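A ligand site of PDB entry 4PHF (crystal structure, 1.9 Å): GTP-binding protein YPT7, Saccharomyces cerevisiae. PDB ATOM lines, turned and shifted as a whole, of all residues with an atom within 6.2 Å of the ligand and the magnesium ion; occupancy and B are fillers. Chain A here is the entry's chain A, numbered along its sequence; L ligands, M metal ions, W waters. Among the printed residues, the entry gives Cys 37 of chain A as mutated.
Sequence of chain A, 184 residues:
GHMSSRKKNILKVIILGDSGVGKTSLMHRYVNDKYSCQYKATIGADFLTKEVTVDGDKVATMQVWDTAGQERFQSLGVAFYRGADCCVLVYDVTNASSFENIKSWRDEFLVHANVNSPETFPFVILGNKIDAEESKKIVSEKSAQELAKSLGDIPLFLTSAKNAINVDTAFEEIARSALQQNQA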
ATOM      1  N   GLY A  17     -13.883 -17.778  15.690  1.00  0.00           N
ATOM      2  CA  GLY A  17     -15.284 -18.209  15.667  1.00  0.00           C
ATOM      3  C   GLY A  17     -15.793 -18.350  14.261  1.00  0.00           C
ATOM      4  O   GLY A  17     -15.202 -17.836  13.278  1.00  0.00           O
ATOM      5  N   ASP A  18     -16.942 -19.035  14.123  1.00  0.00           N
ATOM      6  CA  ASP A  18     -17.452 -19.319  12.790  1.00  0.00           C
ATOM      7  C   ASP A  18     -17.742 -18.036  12.050  1.00  0.00           C
ATOM      8  O   ASP A  18     -18.095 -16.964  12.626  1.00  0.00           O
ATOM      9  CB  ASP A  18     -18.738 -20.220  12.807  1.00  0.00           C
ATOM     10  CG  ASP A  18     -18.507 -21.649  13.364  1.00  0.00           C
ATOM     11  OD1 ASP A  18     -17.378 -22.066  13.661  1.00  0.00           O
ATOM     12  OD2 ASP A  18     -19.529 -22.364  13.525  1.00  0.00           O
ATOM     13  N   SER A  19     -17.716 -18.113  10.724  1.00  0.00           N
ATOM     14  CA  SER A  19     -18.014 -16.915   9.960  1.00  0.00           C
ATOM     15  C   SER A  19     -19.507 -16.601  10.177  1.00  0.00           C
ATOM     16  O   SER A  19     -20.339 -17.479  10.338  1.00  0.00           O
ATOM     17  CB  SER A  19     -17.624 -17.069   8.486  1.00  0.00           C
ATOM     18  OG  SER A  19     -18.623 -17.829   7.856  1.00  0.00           O
ATOM     19  N   GLY A  20     -19.811 -15.305  10.294  1.00  0.00           N
ATOM     20  CA  GLY A  20     -21.195 -14.864  10.406  1.00  0.00           C
ATOM     21  C   GLY A  20     -21.667 -14.548  11.810  1.00  0.00           C
ATOM     22  O   GLY A  20     -22.780 -14.047  11.977  1.00  0.00           O
ATOM     23  N   VAL A  21     -20.803 -14.781  12.805  1.00  0.00           N
ATOM     24  CA  VAL A  21     -21.151 -14.606  14.196  1.00  0.00           C
ATOM     25  C   VAL A  21     -21.057 -13.192  14.704  1.00  0.00           C
ATOM     26  O   VAL A  21     -21.718 -12.883  15.696  1.00  0.00           O
ATOM     27  CB  VAL A  21     -20.316 -15.496  15.169  1.00  0.00           C
ATOM     28  CG1 VAL A  21     -20.544 -16.994  14.876  1.00  0.00           C
ATOM     29  CG2 VAL A  21     -18.850 -15.030  15.247  1.00  0.00           C
ATOM     30  N   GLY A  22     -20.183 -12.370  14.107  1.00  0.00           N
ATOM     31  CA  GLY A  22     -20.117 -10.968  14.430  1.00  0.00           C
ATOM     32  C   GLY A  22     -18.755 -10.525  14.877  1.00  0.00           C
ATOM     33  O   GLY A  22     -18.682  -9.496  15.521  1.00  0.00           O
ATOM     34  N   LYS A  23     -17.717 -11.247  14.461  1.00  0.00           N
ATOM     35  CA  LYS A  23     -16.346 -10.970  14.960  1.00  0.00           C
ATOM     36  C   LYS A  23     -15.911  -9.617  14.482  1.00  0.00           C
ATOM     37  O   LYS A  23     -15.448  -8.791  15.252  1.00  0.00           O
ATOM     38  CB  LYS A  23     -15.341 -12.036  14.457  1.00  0.00           C
ATOM     39  CG  LYS A  23     -15.602 -13.442  14.979  1.00  0.00           C
ATOM     40  CD  LYS A  23     -14.598 -14.503  14.398  1.00  0.00           C
ATOM     41  CE  LYS A  23     -14.558 -14.650  12.887  1.00  0.00           C
ATOM     42  NZ  LYS A  23     -15.913 -15.073  12.302  1.00  0.00           N
ATOM     43  N   THR A  24     -16.067  -9.389  13.198  1.00  0.00           N
ATOM     44  CA  THR A  24     -15.736  -8.067  12.590  1.00  0.00           C
ATOM     45  C   THR A  24     -16.519  -6.874  13.184  1.00  0.00           C
ATOM     46  O   THR A  24     -15.929  -5.771  13.425  1.00  0.00           O
ATOM     47  CB  THR A  24     -15.864  -8.092  11.027  1.00  0.00           C
ATOM     48  OG1 THR A  24     -15.056  -9.182  10.504  1.00  0.00           O
ATOM     49  CG2 THR A  24     -15.366  -6.751  10.429  1.00  0.00           C
ATOM     50  N   SER A  25     -17.817  -7.081  13.349  1.00  0.00           N
ATOM     51  CA  SER A  25     -18.751  -6.113  14.033  1.00  0.00           C
ATOM     52  C   SER A  25     -18.333  -5.792  15.470  1.00  0.00           C
ATOM     53  O   SER A  25     -18.378  -4.663  15.877  1.00  0.00           O
ATOM     54  CB  SER A  25     -20.179  -6.639  14.012  1.00  0.00           C
ATOM     55  OG  SER A  25     -20.589  -6.958  12.682  1.00  0.00           O
ATOM     56  N   LEU A  26     -17.893  -6.802  16.226  1.00  0.00           N
ATOM     57  CA  LEU A  26     -17.503  -6.593  17.608  1.00  0.00           C
ATOM     58  C   LEU A  26     -16.207  -5.783  17.614  1.00  0.00           C
ATOM     59  O   LEU A  26     -16.063  -4.834  18.393  1.00  0.00           O
ATOM     60  CB  LEU A  26     -17.244  -7.887  18.324  1.00  0.00           C
ATOM     61  CG  LEU A  26     -18.497  -8.652  18.766  1.00  0.00           C
ATOM     62  CD1 LEU A  26     -18.202 -10.139  18.995  1.00  0.00           C
ATOM     63  CD2 LEU A  26     -19.063  -7.960  19.982  1.00  0.00           C
ATOM     64  N   TYR A  35     -21.406   0.895  14.315  1.00  0.00           N
ATOM     65  CA  TYR A  35     -21.978  -0.306  13.702  1.00  0.00           C
ATOM     66  C   TYR A  35     -22.799   0.118  12.519  1.00  0.00           C
ATOM     67  O   TYR A  35     -23.556   1.085  12.629  1.00  0.00           O
ATOM     68  CB  TYR A  35     -22.894  -1.060  14.673  1.00  0.00           C
ATOM     69  CG  TYR A  35     -23.691  -2.161  13.996  1.00  0.00           C
ATOM     70  CD1 TYR A  35     -23.237  -3.478  13.969  1.00  0.00           C
ATOM     71  CD2 TYR A  35     -24.913  -1.883  13.375  1.00  0.00           C
ATOM     72  CE1 TYR A  35     -23.962  -4.469  13.332  1.00  0.00           C
ATOM     73  CE2 TYR A  35     -25.645  -2.870  12.750  1.00  0.00           C
ATOM     74  CZ  TYR A  35     -25.176  -4.160  12.740  1.00  0.00           C
ATOM     75  OH  TYR A  35     -25.872  -5.122  12.113  1.00  0.00           O
ATOM     76  N   SER A  36     -22.625  -0.567  11.384  1.00  0.00           N
ATOM     77  CA  SER A  36     -23.533  -0.426  10.192  1.00  0.00           C
ATOM     78  C   SER A  36     -23.997  -1.778   9.764  1.00  0.00           C
ATOM     79  O   SER A  36     -23.209  -2.720   9.743  1.00  0.00           O
ATOM     80  CB  SER A  36     -22.817   0.159   8.950  1.00  0.00           C
ATOM     81  OG  SER A  36     -22.456   1.481   9.144  1.00  0.00           O
ATOM     82  N   CYS A  37     -25.251  -1.871   9.389  1.00  0.00           N
ATOM     83  CA  CYS A  37     -25.715  -2.975   8.551  1.00  0.00           C
ATOM     84  C   CYS A  37     -24.816  -3.095   7.319  1.00  0.00           C
ATOM     85  O   CYS A  37     -24.371  -4.199   6.988  1.00  0.00           O
ATOM     86  CB  CYS A  37     -27.172  -2.755   8.126  1.00  0.00           C
ATOM     87  SG  CYS A  37     -28.270  -2.339   9.519  1.00  0.00           S
ATOM     88  N   ASP A  66      -8.304 -10.080  13.536  1.00  0.00           N
ATOM     89  CA  ASP A  66      -9.563 -10.627  13.079  1.00  0.00           C
ATOM     90  C   ASP A  66      -9.145 -11.683  12.018  1.00  0.00           C
ATOM     91  O   ASP A  66      -7.948 -11.911  11.750  1.00  0.00           O
ATOM     92  CB  ASP A  66     -10.402  -9.442  12.550  1.00  0.00           C
ATOM     93  CG  ASP A  66     -11.885  -9.799  12.192  1.00  0.00           C
ATOM     94  OD1 ASP A  66     -12.362 -10.898  12.496  1.00  0.00           O
ATOM     95  OD2 ASP A  66     -12.581  -8.927  11.608  1.00  0.00           O
ATOM     96  N   THR A  67     -10.097 -12.396  11.446  1.00  0.00           N
ATOM     97  CA  THR A  67      -9.764 -13.623  10.714  1.00  0.00           C
ATOM     98  C   THR A  67      -9.470 -13.309   9.238  1.00  0.00           C
ATOM     99  O   THR A  67     -10.222 -12.573   8.581  1.00  0.00           O
ATOM    100  CB  THR A  67     -10.927 -14.663  10.845  1.00  0.00           C
ATOM    101  OG1 THR A  67     -11.127 -15.000  12.248  1.00  0.00           O
ATOM    102  CG2 THR A  67     -10.633 -15.919  10.020  1.00  0.00           C
ATOM    103  N   ASN A 128     -22.815 -13.480  21.012  1.00  0.00           N
ATOM    104  CA  ASN A 128     -23.194 -12.236  20.348  1.00  0.00           C
ATOM    105  C   ASN A 128     -24.595 -12.350  19.768  1.00  0.00           C
ATOM    106  O   ASN A 128     -25.112 -13.449  19.545  1.00  0.00           O
ATOM    107  CB  ASN A 128     -22.152 -11.928  19.213  1.00  0.00           C
ATOM    108  CG  ASN A 128     -22.266 -10.536  18.627  1.00  0.00           C
ATOM    109  OD1 ASN A 128     -22.214 -10.332  17.340  1.00  0.00           O
ATOM    110  ND2 ASN A 128     -22.430  -9.569  19.476  1.00  0.00           N
ATOM    111  N   LYS A 129     -25.152 -11.170  19.516  1.00  0.00           N
ATOM    112  CA  LYS A 129     -26.439 -10.915  18.903  1.00  0.00           C
ATOM    113  C   LYS A 129     -27.559 -11.023  19.943  1.00  0.00           C
ATOM    114  O   LYS A 129     -28.673 -11.418  19.610  1.00  0.00           O
ATOM    115  CB  LYS A 129     -26.677 -11.773  17.692  1.00  0.00           C
ATOM    116  CG  LYS A 129     -25.558 -11.774  16.640  1.00  0.00           C
ATOM    117  CD  LYS A 129     -26.044 -12.144  15.243  1.00  0.00           C
ATOM    118  CE  LYS A 129     -24.884 -12.393  14.310  1.00  0.00           C
ATOM    119  NZ  LYS A 129     -25.282 -12.981  12.977  1.00  0.00           N
ATOM    120  N   ILE A 130     -27.240 -10.681  21.186  1.00  0.00           N
ATOM    121  CA  ILE A 130     -28.202 -10.807  22.319  1.00  0.00           C
ATOM    122  C   ILE A 130     -29.413  -9.808  22.177  1.00  0.00           C
ATOM    123  O   ILE A 130     -30.414  -9.904  22.903  1.00  0.00           O
ATOM    124  CB  ILE A 130     -27.471 -10.643  23.693  1.00  0.00           C
ATOM    125  CG1 ILE A 130     -28.280 -11.206  24.880  1.00  0.00           C
ATOM    126  CG2 ILE A 130     -27.143  -9.214  23.948  1.00  0.00           C
ATOM    127  CD1 ILE A 130     -28.710 -12.674  24.779  1.00  0.00           C
ATOM    128  N   ASP A 131     -29.300  -8.893  21.224  1.00  0.00           N
ATOM    129  CA  ASP A 131     -30.349  -7.975  20.854  1.00  0.00           C
ATOM    130  C   ASP A 131     -31.435  -8.669  20.032  1.00  0.00           C
ATOM    131  O   ASP A 131     -32.417  -8.031  19.782  1.00  0.00           O
ATOM    132  CB  ASP A 131     -29.800  -6.795  20.009  1.00  0.00           C
ATOM    133  CG  ASP A 131     -29.164  -7.263  18.697  1.00  0.00           C
ATOM    134  OD1 ASP A 131     -29.871  -7.393  17.669  1.00  0.00           O
ATOM    135  OD2 ASP A 131     -27.958  -7.595  18.744  1.00  0.00           O
ATOM    136  N   ALA A 132     -31.254  -9.947  19.621  1.00  0.00           N
ATOM    137  CA  ALA A 132     -32.194 -10.569  18.674  1.00  0.00           C
ATOM    138  C   ALA A 132     -33.505 -10.830  19.383  1.00  0.00           C
ATOM    139  O   ALA A 132     -33.522 -11.068  20.556  1.00  0.00           O
ATOM    140  CB  ALA A 132     -31.660 -11.876  18.138  1.00  0.00           C
ATOM    141  N   THR A 159     -23.308 -10.480  24.349  1.00  0.00           N
ATOM    142  CA  THR A 159     -23.088  -9.174  23.685  1.00  0.00           C
ATOM    143  C   THR A 159     -23.971  -8.841  22.497  1.00  0.00           C
ATOM    144  O   THR A 159     -24.576  -9.719  21.876  1.00  0.00           O
ATOM    145  CB  THR A 159     -21.638  -9.108  23.166  1.00  0.00           C
ATOM    146  OG1 THR A 159     -21.470 -10.099  22.155  1.00  0.00           O
ATOM    147  CG2 THR A 159     -20.666  -9.388  24.240  1.00  0.00           C
ATOM    148  N   SER A 160     -24.067  -7.526  22.208  1.00  0.00           N
ATOM    149  CA  SER A 160     -24.593  -7.011  20.975  1.00  0.00           C
ATOM    150  C   SER A 160     -23.661  -5.962  20.453  1.00  0.00           C
ATOM    151  O   SER A 160     -23.591  -4.866  20.983  1.00  0.00           O
ATOM    152  CB  SER A 160     -25.980  -6.337  21.106  1.00  0.00           C
ATOM    153  OG  SER A 160     -26.472  -6.033  19.790  1.00  0.00           O
ATOM    154  N   ALA A 161     -22.898  -6.312  19.415  1.00  0.00           N
ATOM    155  CA  ALA A 161     -22.197  -5.308  18.636  1.00  0.00           C
ATOM    156  C   ALA A 161     -23.167  -4.203  18.083  1.00  0.00           C
ATOM    157  O   ALA A 161     -22.846  -2.973  18.023  1.00  0.00           O
ATOM    158  CB  ALA A 161     -21.486  -6.000  17.474  1.00  0.00           C
ATOM    159  N   LYS A 162     -24.327  -4.654  17.652  1.00  0.00           N
ATOM    160  CA  LYS A 162     -25.287  -3.765  17.020  1.00  0.00           C
ATOM    161  C   LYS A 162     -25.769  -2.679  17.956  1.00  0.00           C
ATOM    162  O   LYS A 162     -25.615  -1.454  17.616  1.00  0.00           O
ATOM    163  CB  LYS A 162     -26.484  -4.533  16.458  1.00  0.00           C
ATOM    164  CG  LYS A 162     -27.558  -3.637  15.806  1.00  0.00           C
ATOM    165  CD  LYS A 162     -28.649  -4.504  15.226  1.00  0.00           C
ATOM    166  CE  LYS A 162     -29.777  -3.654  14.630  1.00  0.00           C
ATOM    167  NZ  LYS A 162     -30.643  -3.190  15.718  1.00  0.00           N
ATOM    168  N   ASN A 163     -26.283  -3.088  19.128  1.00  0.00           N
ATOM    169  CA  ASN A 163     -26.918  -2.174  20.078  1.00  0.00           C
ATOM    170  C   ASN A 163     -26.009  -1.769  21.238  1.00  0.00           C
ATOM    171  O   ASN A 163     -26.449  -1.104  22.190  1.00  0.00           O
ATOM    172  CB  ASN A 163     -28.222  -2.764  20.603  1.00  0.00           C
ATOM    173  CG  ASN A 163     -29.332  -2.706  19.565  1.00  0.00           C
ATOM    174  OD1 ASN A 163     -30.483  -3.127  19.821  1.00  0.00           O
ATOM    175  ND2 ASN A 163     -29.023  -2.111  18.404  1.00  0.00           N
HETATM  176  O1  LIG L   1     -16.939 -11.312  10.984  1.00  0.00           O
HETATM  177  P1  LIG L   1     -17.946 -12.361  11.051  1.00  0.00           P
HETATM  178  O2  LIG L   1     -17.927 -13.190  12.274  1.00  0.00           O
HETATM  179  O3  LIG L   1     -18.266 -13.096   9.807  1.00  0.00           O
HETATM  180  O4  LIG L   1     -19.362 -11.584  11.289  1.00  0.00           O
HETATM  181  P2  LIG L   1     -19.786 -10.036  10.938  1.00  0.00           P
HETATM  182  O5  LIG L   1     -19.514  -9.712   9.497  1.00  0.00           O
HETATM  183  O6  LIG L   1     -19.296  -9.067  11.940  1.00  0.00           O
HETATM  184  O7  LIG L   1     -21.347 -10.116  10.942  1.00  0.00           O
HETATM  185  C1  LIG L   1     -22.089 -10.999  10.128  1.00  0.00           C
HETATM  186  C2  LIG L   1     -23.536 -10.535  10.169  1.00  0.00           C
HETATM  187  O8  LIG L   1     -23.941 -10.448  11.593  1.00  0.00           O
HETATM  188  C3  LIG L   1     -23.779  -9.119   9.626  1.00  0.00           C
HETATM  189  O9  LIG L   1     -25.121  -9.063   9.103  1.00  0.00           O
HETATM  190  C4  LIG L   1     -23.761  -8.224  10.879  1.00  0.00           C
HETATM  191  O10 LIG L   1     -24.506  -6.995  10.693  1.00  0.00           O
HETATM  192  C5  LIG L   1     -24.513  -9.183  11.844  1.00  0.00           C
HETATM  193  N1  LIG L   1     -24.311  -8.825  13.266  1.00  0.00           N
HETATM  194  C6  LIG L   1     -25.225  -8.638  14.231  1.00  0.00           C
HETATM  195  N2  LIG L   1     -26.559  -8.737  14.157  1.00  0.00           N
HETATM  196  C7  LIG L   1     -23.100  -8.668  13.794  1.00  0.00           C
HETATM  197  N3  LIG L   1     -23.280  -8.335  15.074  1.00  0.00           N
HETATM  198  C8  LIG L   1     -24.584  -8.317  15.404  1.00  0.00           C
HETATM  199  C9  LIG L   1     -25.264  -8.062  16.570  1.00  0.00           C
HETATM  200  O11 LIG L   1     -24.796  -7.736  17.720  1.00  0.00           O
HETATM  201  N4  LIG L   1     -26.650  -8.152  16.444  1.00  0.00           N
HETATM  202  C10 LIG L   1     -27.314  -8.458  15.228  1.00  0.00           C
HETATM  203  N5  LIG L   1     -28.626  -8.569  15.222  1.00  0.00           N
HETATM  204  C11 LIG L   1     -29.475  -8.919  14.058  1.00  0.00           C
HETATM  205  C12 LIG L   1     -29.677  -7.614  13.315  1.00  0.00           C
HETATM  206  C13 LIG L   1     -29.997  -7.987  11.825  1.00  0.00           C
HETATM  207  N6  LIG L   1     -30.108  -6.738  11.025  1.00  0.00           N
HETATM  208  C14 LIG L   1     -29.131  -6.253  10.201  1.00  0.00           C
HETATM  209  O12 LIG L   1     -28.096  -6.845   9.935  1.00  0.00           O
HETATM  210  C15 LIG L   1     -29.482  -4.955   9.446  1.00  0.00           C
HETATM  211  C16 LIG L   1     -28.823  -3.737  10.166  1.00  0.00           C
HETATM  212 MG    MG M   1     -15.514 -10.870   9.645  1.00  0.00          MG
HETATM  213  O   HOH W   1     -19.528 -12.954   7.733  1.00  0.00           O
HETATM  214  O   HOH W   2     -16.823  -9.915   8.432  1.00  0.00           O
HETATM  215  O   HOH W   3     -13.814 -10.405   8.239  1.00  0.00           O
HETATM  216  O   HOH W   4     -13.884 -11.819  10.815  1.00  0.00           O
HETATM  217  O   HOH W   5     -15.798 -12.713   8.707  1.00  0.00           O
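One residue has an atom within 4 Å of the magnesium ion: Thr 24. The nearest printed residue that does not touch the magnesium ion is Asp 66 (4.03 Å).
Residues that only touch the ligand: Asp 18 (3.8 Å) and Ser 19 (3.7 Å). Hydrophobic or aromatic side chains within 4 Å of the ligand: Val 21, Tyr 35 and Ala 161. 16 residues have an atom within 4 Å of the ligand: Asp 18, Ser 19, Gly 20, Val 21, Gly 22, Lys 23, Thr 24, Ser 25, Tyr 35, Cys 37, Asn 128, Lys 129, Asp 131, Ser 160, Ala 161 and Lys 162.
The magnesium ion is bound by the side-chain hydroxyl (OG1) of Thr 24, 1.9 Å away. An oxygen (O1) of the ligand binds the magnesium ion. Water W2 binds the magnesium ion (2.0 Å). Water W5 binds the magnesium ion, at 2.1 Å. Water W4 is bound to the magnesium ion (2.2 Å). The magnesium ion is bound by water W3.
A carbon (C16) of the ligand is bonded to the side-chain sulfur (SG) of Cys 37, 1.6 Å away. N of Thr 24 sits at hydrogen-bond distance from O6 of the ligand. The backbone NH (N) of Ser 25 is in hydrogen-bond range of an oxygen (O6) of the ligand. OG of Ser 25 is in hydrogen-bond range of O6 of the ligand, 2.6 Å away. The side-chain carboxylate of Asp 131 sits at hydrogen-bond distance from a nitrogen (N4) of the ligand (2.7 Å). An oxygen (O10) of the ligand is in hydrogen-bond range of the side-chain hydroxyl (OH) of Tyr 35, 2.7 Å away. The backbone NH (N) of Gly 20 is in hydrogen-bond range of an oxygen (O3) of the ligand (2.7 Å). The backbone NH (N) of Lys 23 lies within hydrogen-bond range of an oxygen (O2) of the ligand. The side-chain amino group (NZ) of Lys 23 is in salt-bridge range of an oxygen (O2) of the ligand (2.8 Å). An oxygen (O11) of the ligand sits at hydrogen-bond distance from the backbone NH of Ala 161 (2.9 Å). O2 of the ligand is in hydrogen-bond range of N of Gly 22 (3.0 Å). The backbone NH (N) of Lys 162 lies within hydrogen-bond range of an oxygen (O11) of the ligand (3.1 Å). The side-chain hydroxyl (OG) of Ser 160 is in hydrogen-bond range of an oxygen (O11) of the ligand. O8 of the ligand is in hydrogen-bond range of NZ of Lys 129, 3.2 Å away. The side-chain amide oxygen of Asn 128 sits close to a nitrogen (N3) of the ligand, at 3.2 Å. An oxygen (O2) of the ligand lies within hydrogen-bond range of the backbone NH (N) of Val 21.
The side-chain carboxylate (OD2) of Asp 66 sits close to the side-chain hydroxyl (OG1) of Thr 24 (2.7 Å). The backbone carbonyl oxygen (O) of Gly 20 is in hydrogen-bond range of the side-chain amino group (NZ) of Lys 129, 2.9 Å away. O of Gly 17 is in hydrogen-bond range of NZ of Lys 23 (3.0 Å). The backbone NH (N) of Ala 161 lies close to the side-chain amide nitrogen (ND2) of Asn 128 (3.3 Å). The backbone NH (N) of Lys 162 sits close to the side-chain hydroxyl (OG) of Ser 160. The side-chain amide nitrogen (ND2) of Asn 163 lies close to the side-chain amino group (NZ) of Lys 162, at 3.3 Å. The backbone NH of Asn 163 sits at hydrogen-bond distance from the side-chain hydroxyl of Ser 160, at 3.0 Å. N of Lys 129 sits at hydrogen-bond distance from O of Thr 159 (2.8 Å).
Water W1 lies within hydrogen-bond range of O3 of the ligand (2.4 Å) and N of Gly 20 (3.5 Å).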
